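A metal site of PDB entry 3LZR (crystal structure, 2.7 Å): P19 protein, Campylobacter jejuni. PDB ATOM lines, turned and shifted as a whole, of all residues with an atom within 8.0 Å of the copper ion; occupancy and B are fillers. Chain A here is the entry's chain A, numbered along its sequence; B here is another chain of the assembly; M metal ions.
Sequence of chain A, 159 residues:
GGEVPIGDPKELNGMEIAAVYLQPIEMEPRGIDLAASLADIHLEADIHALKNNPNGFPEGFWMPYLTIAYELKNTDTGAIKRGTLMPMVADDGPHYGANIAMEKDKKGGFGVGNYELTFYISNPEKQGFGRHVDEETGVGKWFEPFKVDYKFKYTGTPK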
ATOM      1  N   LEU A  22      -8.590 -10.256  14.438  1.00  0.00           N
ATOM      2  CA  LEU A  22      -9.428  -9.845  15.570  1.00  0.00           C
ATOM      3  C   LEU A  22      -9.420 -10.924  16.641  1.00  0.00           C
ATOM      4  O   LEU A  22      -8.724 -11.934  16.516  1.00  0.00           O
ATOM      5  CB  LEU A  22     -10.856  -9.545  15.083  1.00  0.00           C
ATOM      6  CG  LEU A  22     -11.555 -10.632  14.248  1.00  0.00           C
ATOM      7  CD1 LEU A  22     -13.068 -10.460  14.306  1.00  0.00           C
ATOM      8  CD2 LEU A  22     -11.069 -10.613  12.804  1.00  0.00           C
ATOM      9  N   GLN A  23     -10.180 -10.723  17.714  1.00  0.00           N
ATOM     10  CA  GLN A  23     -10.289 -11.705  18.800  1.00  0.00           C
ATOM     11  C   GLN A  23     -10.725 -13.074  18.261  1.00  0.00           C
ATOM     12  O   GLN A  23     -11.424 -13.155  17.250  1.00  0.00           O
ATOM     13  CB  GLN A  23     -11.262 -11.225  19.892  1.00  0.00           C
ATOM     14  CG  GLN A  23     -12.757 -11.231  19.533  1.00  0.00           C
ATOM     15  CD  GLN A  23     -13.201 -10.048  18.669  1.00  0.00           C
ATOM     16  OE1 GLN A  23     -12.397  -9.174  18.309  1.00  0.00           O
ATOM     17  NE2 GLN A  23     -14.492 -10.003  18.353  1.00  0.00           N
ATOM     18  N   ILE A  25     -12.730 -16.465  17.546  1.00  0.00           N
ATOM     19  CA  ILE A  25     -14.172 -16.633  17.334  1.00  0.00           C
ATOM     20  C   ILE A  25     -14.578 -18.107  17.386  1.00  0.00           C
ATOM     21  O   ILE A  25     -13.785 -18.979  17.029  1.00  0.00           O
ATOM     22  CB  ILE A  25     -14.630 -15.996  15.989  1.00  0.00           C
ATOM     23  CG1 ILE A  25     -14.022 -16.727  14.771  1.00  0.00           C
ATOM     24  CG2 ILE A  25     -14.277 -14.519  15.951  1.00  0.00           C
ATOM     25  CD1 ILE A  25     -14.880 -17.884  14.233  1.00  0.00           C
ATOM     26  N   GLU A  26     -15.805 -18.357  17.835  1.00  0.00           N
ATOM     27  CA  GLU A  26     -16.375 -19.699  17.872  1.00  0.00           C
ATOM     28  C   GLU A  26     -17.042 -19.986  16.526  1.00  0.00           C
ATOM     29  O   GLU A  26     -17.875 -19.217  16.061  1.00  0.00           O
ATOM     30  CB  GLU A  26     -17.436 -19.800  18.979  1.00  0.00           C
ATOM     31  CG  GLU A  26     -16.930 -19.457  20.380  1.00  0.00           C
ATOM     32  CD  GLU A  26     -18.024 -19.485  21.429  1.00  0.00           C
ATOM     33  OE1 GLU A  26     -19.165 -19.898  21.099  1.00  0.00           O
ATOM     34  OE2 GLU A  26     -17.753 -19.113  22.589  1.00  0.00           O
ATOM     35  N   MET A  27     -16.669 -21.105  15.896  1.00  0.00           N
ATOM     36  CA  MET A  27     -17.191 -21.463  14.570  1.00  0.00           C
ATOM     37  C   MET A  27     -17.933 -22.806  14.572  1.00  0.00           C
ATOM     38  O   MET A  27     -17.454 -23.784  15.144  1.00  0.00           O
ATOM     39  CB  MET A  27     -16.051 -21.525  13.548  1.00  0.00           C
ATOM     40  CG  MET A  27     -16.520 -21.476  12.089  1.00  0.00           C
ATOM     41  SD  MET A  27     -15.285 -22.020  10.876  1.00  0.00           S
ATOM     42  CE  MET A  27     -15.336 -23.790  11.100  1.00  0.00           C
ATOM     43  N   ASP A  33     -12.018 -26.023  12.811  1.00  0.00           N
ATOM     44  CA  ASP A  33     -11.153 -24.920  13.217  1.00  0.00           C
ATOM     45  C   ASP A  33     -10.574 -25.128  14.624  1.00  0.00           C
ATOM     46  O   ASP A  33     -11.074 -25.940  15.402  1.00  0.00           O
ATOM     47  CB  ASP A  33     -11.948 -23.595  13.168  1.00  0.00           C
ATOM     48  CG  ASP A  33     -11.059 -22.356  13.143  1.00  0.00           C
ATOM     49  OD1 ASP A  33      -9.911 -22.431  12.636  1.00  0.00           O
ATOM     50  OD2 ASP A  33     -11.515 -21.303  13.624  1.00  0.00           O
ATOM     51  N   HIS A  42      -7.886 -14.309  15.388  1.00  0.00           N
ATOM     52  CA  HIS A  42      -8.606 -14.889  14.250  1.00  0.00           C
ATOM     53  C   HIS A  42      -8.169 -14.162  12.987  1.00  0.00           C
ATOM     54  O   HIS A  42      -8.486 -12.990  12.799  1.00  0.00           O
ATOM     55  CB  HIS A  42     -10.123 -14.746  14.447  1.00  0.00           C
ATOM     56  CG  HIS A  42     -10.926 -15.407  13.383  1.00  0.00           C
ATOM     57  ND1 HIS A  42     -11.046 -16.771  13.277  1.00  0.00           N
ATOM     58  CD2 HIS A  42     -11.680 -14.889  12.372  1.00  0.00           C
ATOM     59  CE1 HIS A  42     -11.811 -17.079  12.252  1.00  0.00           C
ATOM     60  NE2 HIS A  42     -12.208 -15.947  11.684  1.00  0.00           N
ATOM     61  N   LEU A  43      -7.401 -14.850  12.137  1.00  0.00           N
ATOM     62  CA  LEU A  43      -6.919 -14.269  10.884  1.00  0.00           C
ATOM     63  C   LEU A  43      -8.033 -14.293   9.838  1.00  0.00           C
ATOM     64  O   LEU A  43      -8.773 -15.278   9.757  1.00  0.00           O
ATOM     65  CB  LEU A  43      -5.689 -15.031  10.380  1.00  0.00           C
ATOM     66  CG  LEU A  43      -4.923 -14.416   9.205  1.00  0.00           C
ATOM     67  CD1 LEU A  43      -4.372 -13.042   9.552  1.00  0.00           C
ATOM     68  CD2 LEU A  43      -3.806 -15.350   8.770  1.00  0.00           C
ATOM     69  N   GLU A  44      -8.148 -13.222   9.063  1.00  0.00           N
ATOM     70  CA  GLU A  44      -9.151 -13.147   7.993  1.00  0.00           C
ATOM     71  C   GLU A  44      -8.549 -12.637   6.698  1.00  0.00           C
ATOM     72  O   GLU A  44      -7.750 -11.694   6.694  1.00  0.00           O
ATOM     73  CB  GLU A  44     -10.325 -12.240   8.405  1.00  0.00           C
ATOM     74  CG  GLU A  44     -11.186 -12.803   9.527  1.00  0.00           C
ATOM     75  CD  GLU A  44     -12.448 -11.974   9.785  1.00  0.00           C
ATOM     76  OE1 GLU A  44     -12.676 -10.971   9.077  1.00  0.00           O
ATOM     77  OE2 GLU A  44     -13.219 -12.342  10.697  1.00  0.00           O
ATOM     78  N   ALA A  45      -8.934 -13.270   5.591  1.00  0.00           N
ATOM     79  CA  ALA A  45      -8.594 -12.803   4.245  1.00  0.00           C
ATOM     80  C   ALA A  45      -9.844 -12.253   3.575  1.00  0.00           C
ATOM     81  O   ALA A  45     -10.777 -13.007   3.270  1.00  0.00           O
ATOM     82  CB  ALA A  45      -8.001 -13.938   3.427  1.00  0.00           C
ATOM     83  N   MET A  86     -10.250 -21.251   5.914  1.00  0.00           N
ATOM     84  CA  MET A  86     -11.478 -21.887   5.435  1.00  0.00           C
ATOM     85  C   MET A  86     -12.580 -20.846   5.254  1.00  0.00           C
ATOM     86  O   MET A  86     -12.668 -19.880   6.013  1.00  0.00           O
ATOM     87  CB  MET A  86     -11.937 -22.962   6.426  1.00  0.00           C
ATOM     88  CG  MET A  86     -11.002 -24.175   6.517  1.00  0.00           C
ATOM     89  SD  MET A  86     -11.053 -25.265   5.053  1.00  0.00           S
ATOM     90  CE  MET A  86     -12.682 -26.012   5.224  1.00  0.00           C
ATOM     91  N   PRO A  87     -13.443 -21.035   4.234  1.00  0.00           N
ATOM     92  CA  PRO A  87     -14.547 -20.101   4.005  1.00  0.00           C
ATOM     93  C   PRO A  87     -15.607 -20.164   5.095  1.00  0.00           C
ATOM     94  O   PRO A  87     -15.974 -21.243   5.550  1.00  0.00           O
ATOM     95  CB  PRO A  87     -15.124 -20.569   2.661  1.00  0.00           C
ATOM     96  CG  PRO A  87     -14.754 -21.992   2.570  1.00  0.00           C
ATOM     97  CD  PRO A  87     -13.435 -22.119   3.237  1.00  0.00           C
ATOM     98  N   MET A  88     -16.092 -18.993   5.523  1.00  0.00           N
ATOM     99  CA  MET A  88     -17.123 -18.898   6.551  1.00  0.00           C
ATOM    100  C   MET A  88     -17.807 -17.537   6.479  1.00  0.00           C
ATOM    101  O   MET A  88     -17.328 -16.631   5.800  1.00  0.00           O
ATOM    102  CB  MET A  88     -16.520 -19.107   7.939  1.00  0.00           C
ATOM    103  CG  MET A  88     -15.553 -18.012   8.359  1.00  0.00           C
ATOM    104  SD  MET A  88     -14.572 -18.447   9.803  1.00  0.00           S
ATOM    105  CE  MET A  88     -13.439 -19.638   9.094  1.00  0.00           C
ATOM    106  N   VAL A  89     -18.915 -17.388   7.207  1.00  0.00           N
ATOM    107  CA  VAL A  89     -19.657 -16.137   7.241  1.00  0.00           C
ATOM    108  C   VAL A  89     -19.762 -15.592   8.666  1.00  0.00           C
ATOM    109  O   VAL A  89     -19.865 -16.352   9.627  1.00  0.00           O
ATOM    110  CB  VAL A  89     -21.070 -16.299   6.622  1.00  0.00           C
ATOM    111  CG1 VAL A  89     -21.930 -17.241   7.452  1.00  0.00           C
ATOM    112  CG2 VAL A  89     -21.741 -14.938   6.456  1.00  0.00           C
ATOM    113  N   ALA A  90     -19.699 -14.267   8.782  1.00  0.00           N
ATOM    114  CA  ALA A  90     -19.869 -13.572  10.062  1.00  0.00           C
ATOM    115  C   ALA A  90     -20.900 -12.453   9.886  1.00  0.00           C
ATOM    116  O   ALA A  90     -21.536 -12.373   8.838  1.00  0.00           O
ATOM    117  CB  ALA A  90     -18.532 -13.001  10.532  1.00  0.00           C
ATOM    118  N   ASP A  92     -20.354  -9.374   9.470  1.00  0.00           N
ATOM    119  CA  ASP A  92     -19.875  -8.531   8.382  1.00  0.00           C
ATOM    120  C   ASP A  92     -19.660  -9.328   7.080  1.00  0.00           C
ATOM    121  O   ASP A  92     -18.819  -8.977   6.254  1.00  0.00           O
ATOM    122  CB  ASP A  92     -18.597  -7.766   8.792  1.00  0.00           C
ATOM    123  CG  ASP A  92     -17.415  -8.685   9.101  1.00  0.00           C
ATOM    124  OD1 ASP A  92     -17.579  -9.922   9.113  1.00  0.00           O
ATOM    125  OD2 ASP A  92     -16.309  -8.145   9.339  1.00  0.00           O
ATOM    126  N   GLY A  93     -20.434 -10.394   6.912  1.00  0.00           N
ATOM    127  CA  GLY A  93     -20.439 -11.166   5.672  1.00  0.00           C
ATOM    128  C   GLY A  93     -19.364 -12.229   5.584  1.00  0.00           C
ATOM    129  O   GLY A  93     -18.604 -12.446   6.533  1.00  0.00           O
ATOM    130  N   PRO A  94     -19.288 -12.894   4.410  1.00  0.00           N
ATOM    131  CA  PRO A  94     -18.388 -14.018   4.220  1.00  0.00           C
ATOM    132  C   PRO A  94     -16.922 -13.619   4.125  1.00  0.00           C
ATOM    133  O   PRO A  94     -16.608 -12.501   3.699  1.00  0.00           O
ATOM    134  CB  PRO A  94     -18.858 -14.618   2.898  1.00  0.00           C
ATOM    135  CG  PRO A  94     -19.426 -13.470   2.151  1.00  0.00           C
ATOM    136  CD  PRO A  94     -20.029 -12.566   3.182  1.00  0.00           C
ATOM    137  N   HIS A  95     -16.039 -14.531   4.527  1.00  0.00           N
ATOM    138  CA  HIS A  95     -14.606 -14.338   4.395  1.00  0.00           C
ATOM    139  C   HIS A  95     -13.889 -15.680   4.474  1.00  0.00           C
ATOM    140  O   HIS A  95     -14.526 -16.720   4.631  1.00  0.00           O
ATOM    141  CB  HIS A  95     -14.079 -13.378   5.480  1.00  0.00           C
ATOM    142  CG  HIS A  95     -14.318 -13.855   6.870  1.00  0.00           C
ATOM    143  ND1 HIS A  95     -15.477 -13.588   7.565  1.00  0.00           N
ATOM    144  CD2 HIS A  95     -13.544 -14.579   7.719  1.00  0.00           C
ATOM    145  CE1 HIS A  95     -15.414 -14.127   8.773  1.00  0.00           C
ATOM    146  NE2 HIS A  95     -14.243 -14.730   8.890  1.00  0.00           N
ATOM    147  N   TYR A  96     -12.563 -15.659   4.326  1.00  0.00           N
ATOM    148  CA  TYR A  96     -11.717 -16.823   4.592  1.00  0.00           C
ATOM    149  C   TYR A  96     -10.964 -16.547   5.871  1.00  0.00           C
ATOM    150  O   TYR A  96     -10.319 -15.507   5.993  1.00  0.00           O
ATOM    151  CB  TYR A  96     -10.724 -17.040   3.441  1.00  0.00           C
ATOM    152  CG  TYR A  96     -11.371 -17.391   2.119  1.00  0.00           C
ATOM    153  CD1 TYR A  96     -11.721 -18.695   1.810  1.00  0.00           C
ATOM    154  CD2 TYR A  96     -11.646 -16.393   1.180  1.00  0.00           C
ATOM    155  CE1 TYR A  96     -12.317 -19.018   0.598  1.00  0.00           C
ATOM    156  CE2 TYR A  96     -12.246 -16.697  -0.037  1.00  0.00           C
ATOM    157  CZ  TYR A  96     -12.574 -18.011  -0.319  1.00  0.00           C
ATOM    158  OH  TYR A  96     -13.176 -18.312  -1.523  1.00  0.00           O
ATOM    159  N   GLY A  97     -11.042 -17.460   6.834  1.00  0.00           N
ATOM    160  CA  GLY A  97     -10.386 -17.242   8.122  1.00  0.00           C
ATOM    161  C   GLY A  97      -9.984 -18.495   8.873  1.00  0.00           C
ATOM    162  O   GLY A  97     -10.295 -19.616   8.467  1.00  0.00           O
ATOM    163  N   ALA A  98      -9.284 -18.284   9.978  1.00  0.00           N
ATOM    164  CA  ALA A  98      -8.847 -19.373  10.848  1.00  0.00           C
ATOM    165  C   ALA A  98      -8.373 -18.830  12.192  1.00  0.00           C
ATOM    166  O   ALA A  98      -7.662 -17.828  12.236  1.00  0.00           O
ATOM    167  CB  ALA A  98      -7.728 -20.167  10.177  1.00  0.00           C
ATOM    168  N   ASN A  99      -8.784 -19.481  13.280  1.00  0.00           N
ATOM    169  CA  ASN A  99      -8.221 -19.212  14.596  1.00  0.00           C
ATOM    170  C   ASN A  99      -6.768 -19.670  14.611  1.00  0.00           C
ATOM    171  O   ASN A  99      -6.444 -20.725  14.063  1.00  0.00           O
ATOM    172  CB  ASN A  99      -9.014 -19.921  15.709  1.00  0.00           C
ATOM    173  CG  ASN A  99     -10.326 -19.221  16.035  1.00  0.00           C
ATOM    174  OD1 ASN A  99     -10.597 -18.107  15.588  1.00  0.00           O
ATOM    175  ND2 ASN A  99     -11.150 -19.879  16.840  1.00  0.00           N
ATOM    176  N   GLY B 130     -18.379 -22.624   7.074  1.00  0.00           N
ATOM    177  CA  GLY B 130     -18.535 -22.312   8.489  1.00  0.00           C
ATOM    178  C   GLY B 130     -19.343 -21.060   8.741  1.00  0.00           C
ATOM    179  O   GLY B 130     -19.709 -20.352   7.807  1.00  0.00           O
ATOM    180  N   ARG B 131     -19.616 -20.796  10.013  1.00  0.00           N
ATOM    181  CA  ARG B 131     -20.226 -19.548  10.430  1.00  0.00           C
ATOM    182  C   ARG B 131     -19.797 -19.232  11.864  1.00  0.00           C
ATOM    183  O   ARG B 131     -19.604 -20.142  12.671  1.00  0.00           O
ATOM    184  CB  ARG B 131     -21.751 -19.600  10.320  1.00  0.00           C
ATOM    185  CG  ARG B 131     -22.455 -20.387  11.433  1.00  0.00           C
ATOM    186  CD  ARG B 131     -23.928 -20.589  11.152  1.00  0.00           C
ATOM    187  NE  ARG B 131     -24.536 -21.525  12.100  1.00  0.00           N
ATOM    188  CZ  ARG B 131     -25.047 -21.205  13.286  1.00  0.00           C
ATOM    189  NH1 ARG B 131     -25.050 -19.949  13.717  1.00  0.00           N
ATOM    190  NH2 ARG B 131     -25.559 -22.159  14.052  1.00  0.00           N
ATOM    191  N   HIS B 132     -19.653 -17.940  12.159  1.00  0.00           N
ATOM    192  CA  HIS B 132     -19.339 -17.499  13.513  1.00  0.00           C
ATOM    193  C   HIS B 132     -20.569 -17.649  14.398  1.00  0.00           C
ATOM    194  O   HIS B 132     -21.687 -17.325  13.973  1.00  0.00           O
ATOM    195  CB  HIS B 132     -18.906 -16.032  13.496  1.00  0.00           C
ATOM    196  CG  HIS B 132     -17.583 -15.787  12.834  1.00  0.00           C
ATOM    197  ND1 HIS B 132     -16.776 -14.724  13.168  1.00  0.00           N
ATOM    198  CD2 HIS B 132     -16.923 -16.473  11.868  1.00  0.00           C
ATOM    199  CE1 HIS B 132     -15.679 -14.753  12.425  1.00  0.00           C
ATOM    200  NE2 HIS B 132     -15.751 -15.802  11.630  1.00  0.00           N
ATOM    201  N   ASP B 134     -20.199 -16.734  17.960  1.00  0.00           N
ATOM    202  CA  ASP B 134     -19.932 -15.923  19.157  1.00  0.00           C
ATOM    203  C   ASP B 134     -20.909 -14.744  19.252  1.00  0.00           C
ATOM    204  O   ASP B 134     -21.595 -14.424  18.281  1.00  0.00           O
ATOM    205  CB  ASP B 134     -18.474 -15.429  19.193  1.00  0.00           C
ATOM    206  CG  ASP B 134     -18.075 -14.664  17.945  1.00  0.00           C
ATOM    207  OD1 ASP B 134     -17.969 -15.298  16.870  1.00  0.00           O
ATOM    208  OD2 ASP B 134     -17.859 -13.433  18.028  1.00  0.00           O
ATOM    209  N   THR B 137     -19.625 -11.325  16.983  1.00  0.00           N
ATOM    210  CA  THR B 137     -19.618 -11.398  15.509  1.00  0.00           C
ATOM    211  C   THR B 137     -20.461 -12.543  14.926  1.00  0.00           C
ATOM    212  O   THR B 137     -20.301 -12.886  13.753  1.00  0.00           O
ATOM    213  CB  THR B 137     -18.177 -11.546  14.983  1.00  0.00           C
ATOM    214  OG1 THR B 137     -17.649 -12.826  15.368  1.00  0.00           O
ATOM    215  CG2 THR B 137     -17.273 -10.434  15.515  1.00  0.00           C
HETATM  216 CU    CU M   1     -13.900 -16.228  10.363  1.00  0.00          CU
HETATM  217 MN    MN M   2     -14.028  -8.711   8.757  1.00  0.00          MN
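ND1 of His 42 is in hydrogen-bond range of OD1 of Asn 99, 2.7 Å away. The backbone NH (N) of His 42 is in hydrogen-bond range of the backbone carbonyl oxygen (O) of Leu 22 (2.8 Å). A ring nitrogen (NE2) of His 95 sits close to the side-chain carboxylate (OE2) of Glu 44 (3.2 Å). The backbone carbonyl oxygen of Val 89 is in hydrogen-bond range of the backbone NH of His 132 of chain B (3.0 Å). The backbone carbonyl oxygen of Gly 93 is in hydrogen-bond range of a ring nitrogen (ND1) of His 95, at 3.5 Å. A ring nitrogen (ND1) of His 132 of chain B sits at hydrogen-bond distance from the side-chain hydroxyl (OG1) of Thr 137 of chain B, 3.0 Å away.
Glu 44 touches the copper ion. Of the 28 residues printed, 5 come within 4 Å of the copper ion.
The copper ion is bound by NE2 of His 95 (2.1 Å). The copper ion is bound by NE2 of His 42 (2.2 Å). NE2 of His 132 of chain B is bound to the copper ion. SD of Met 88 binds the copper ion, 2.4 Å away.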
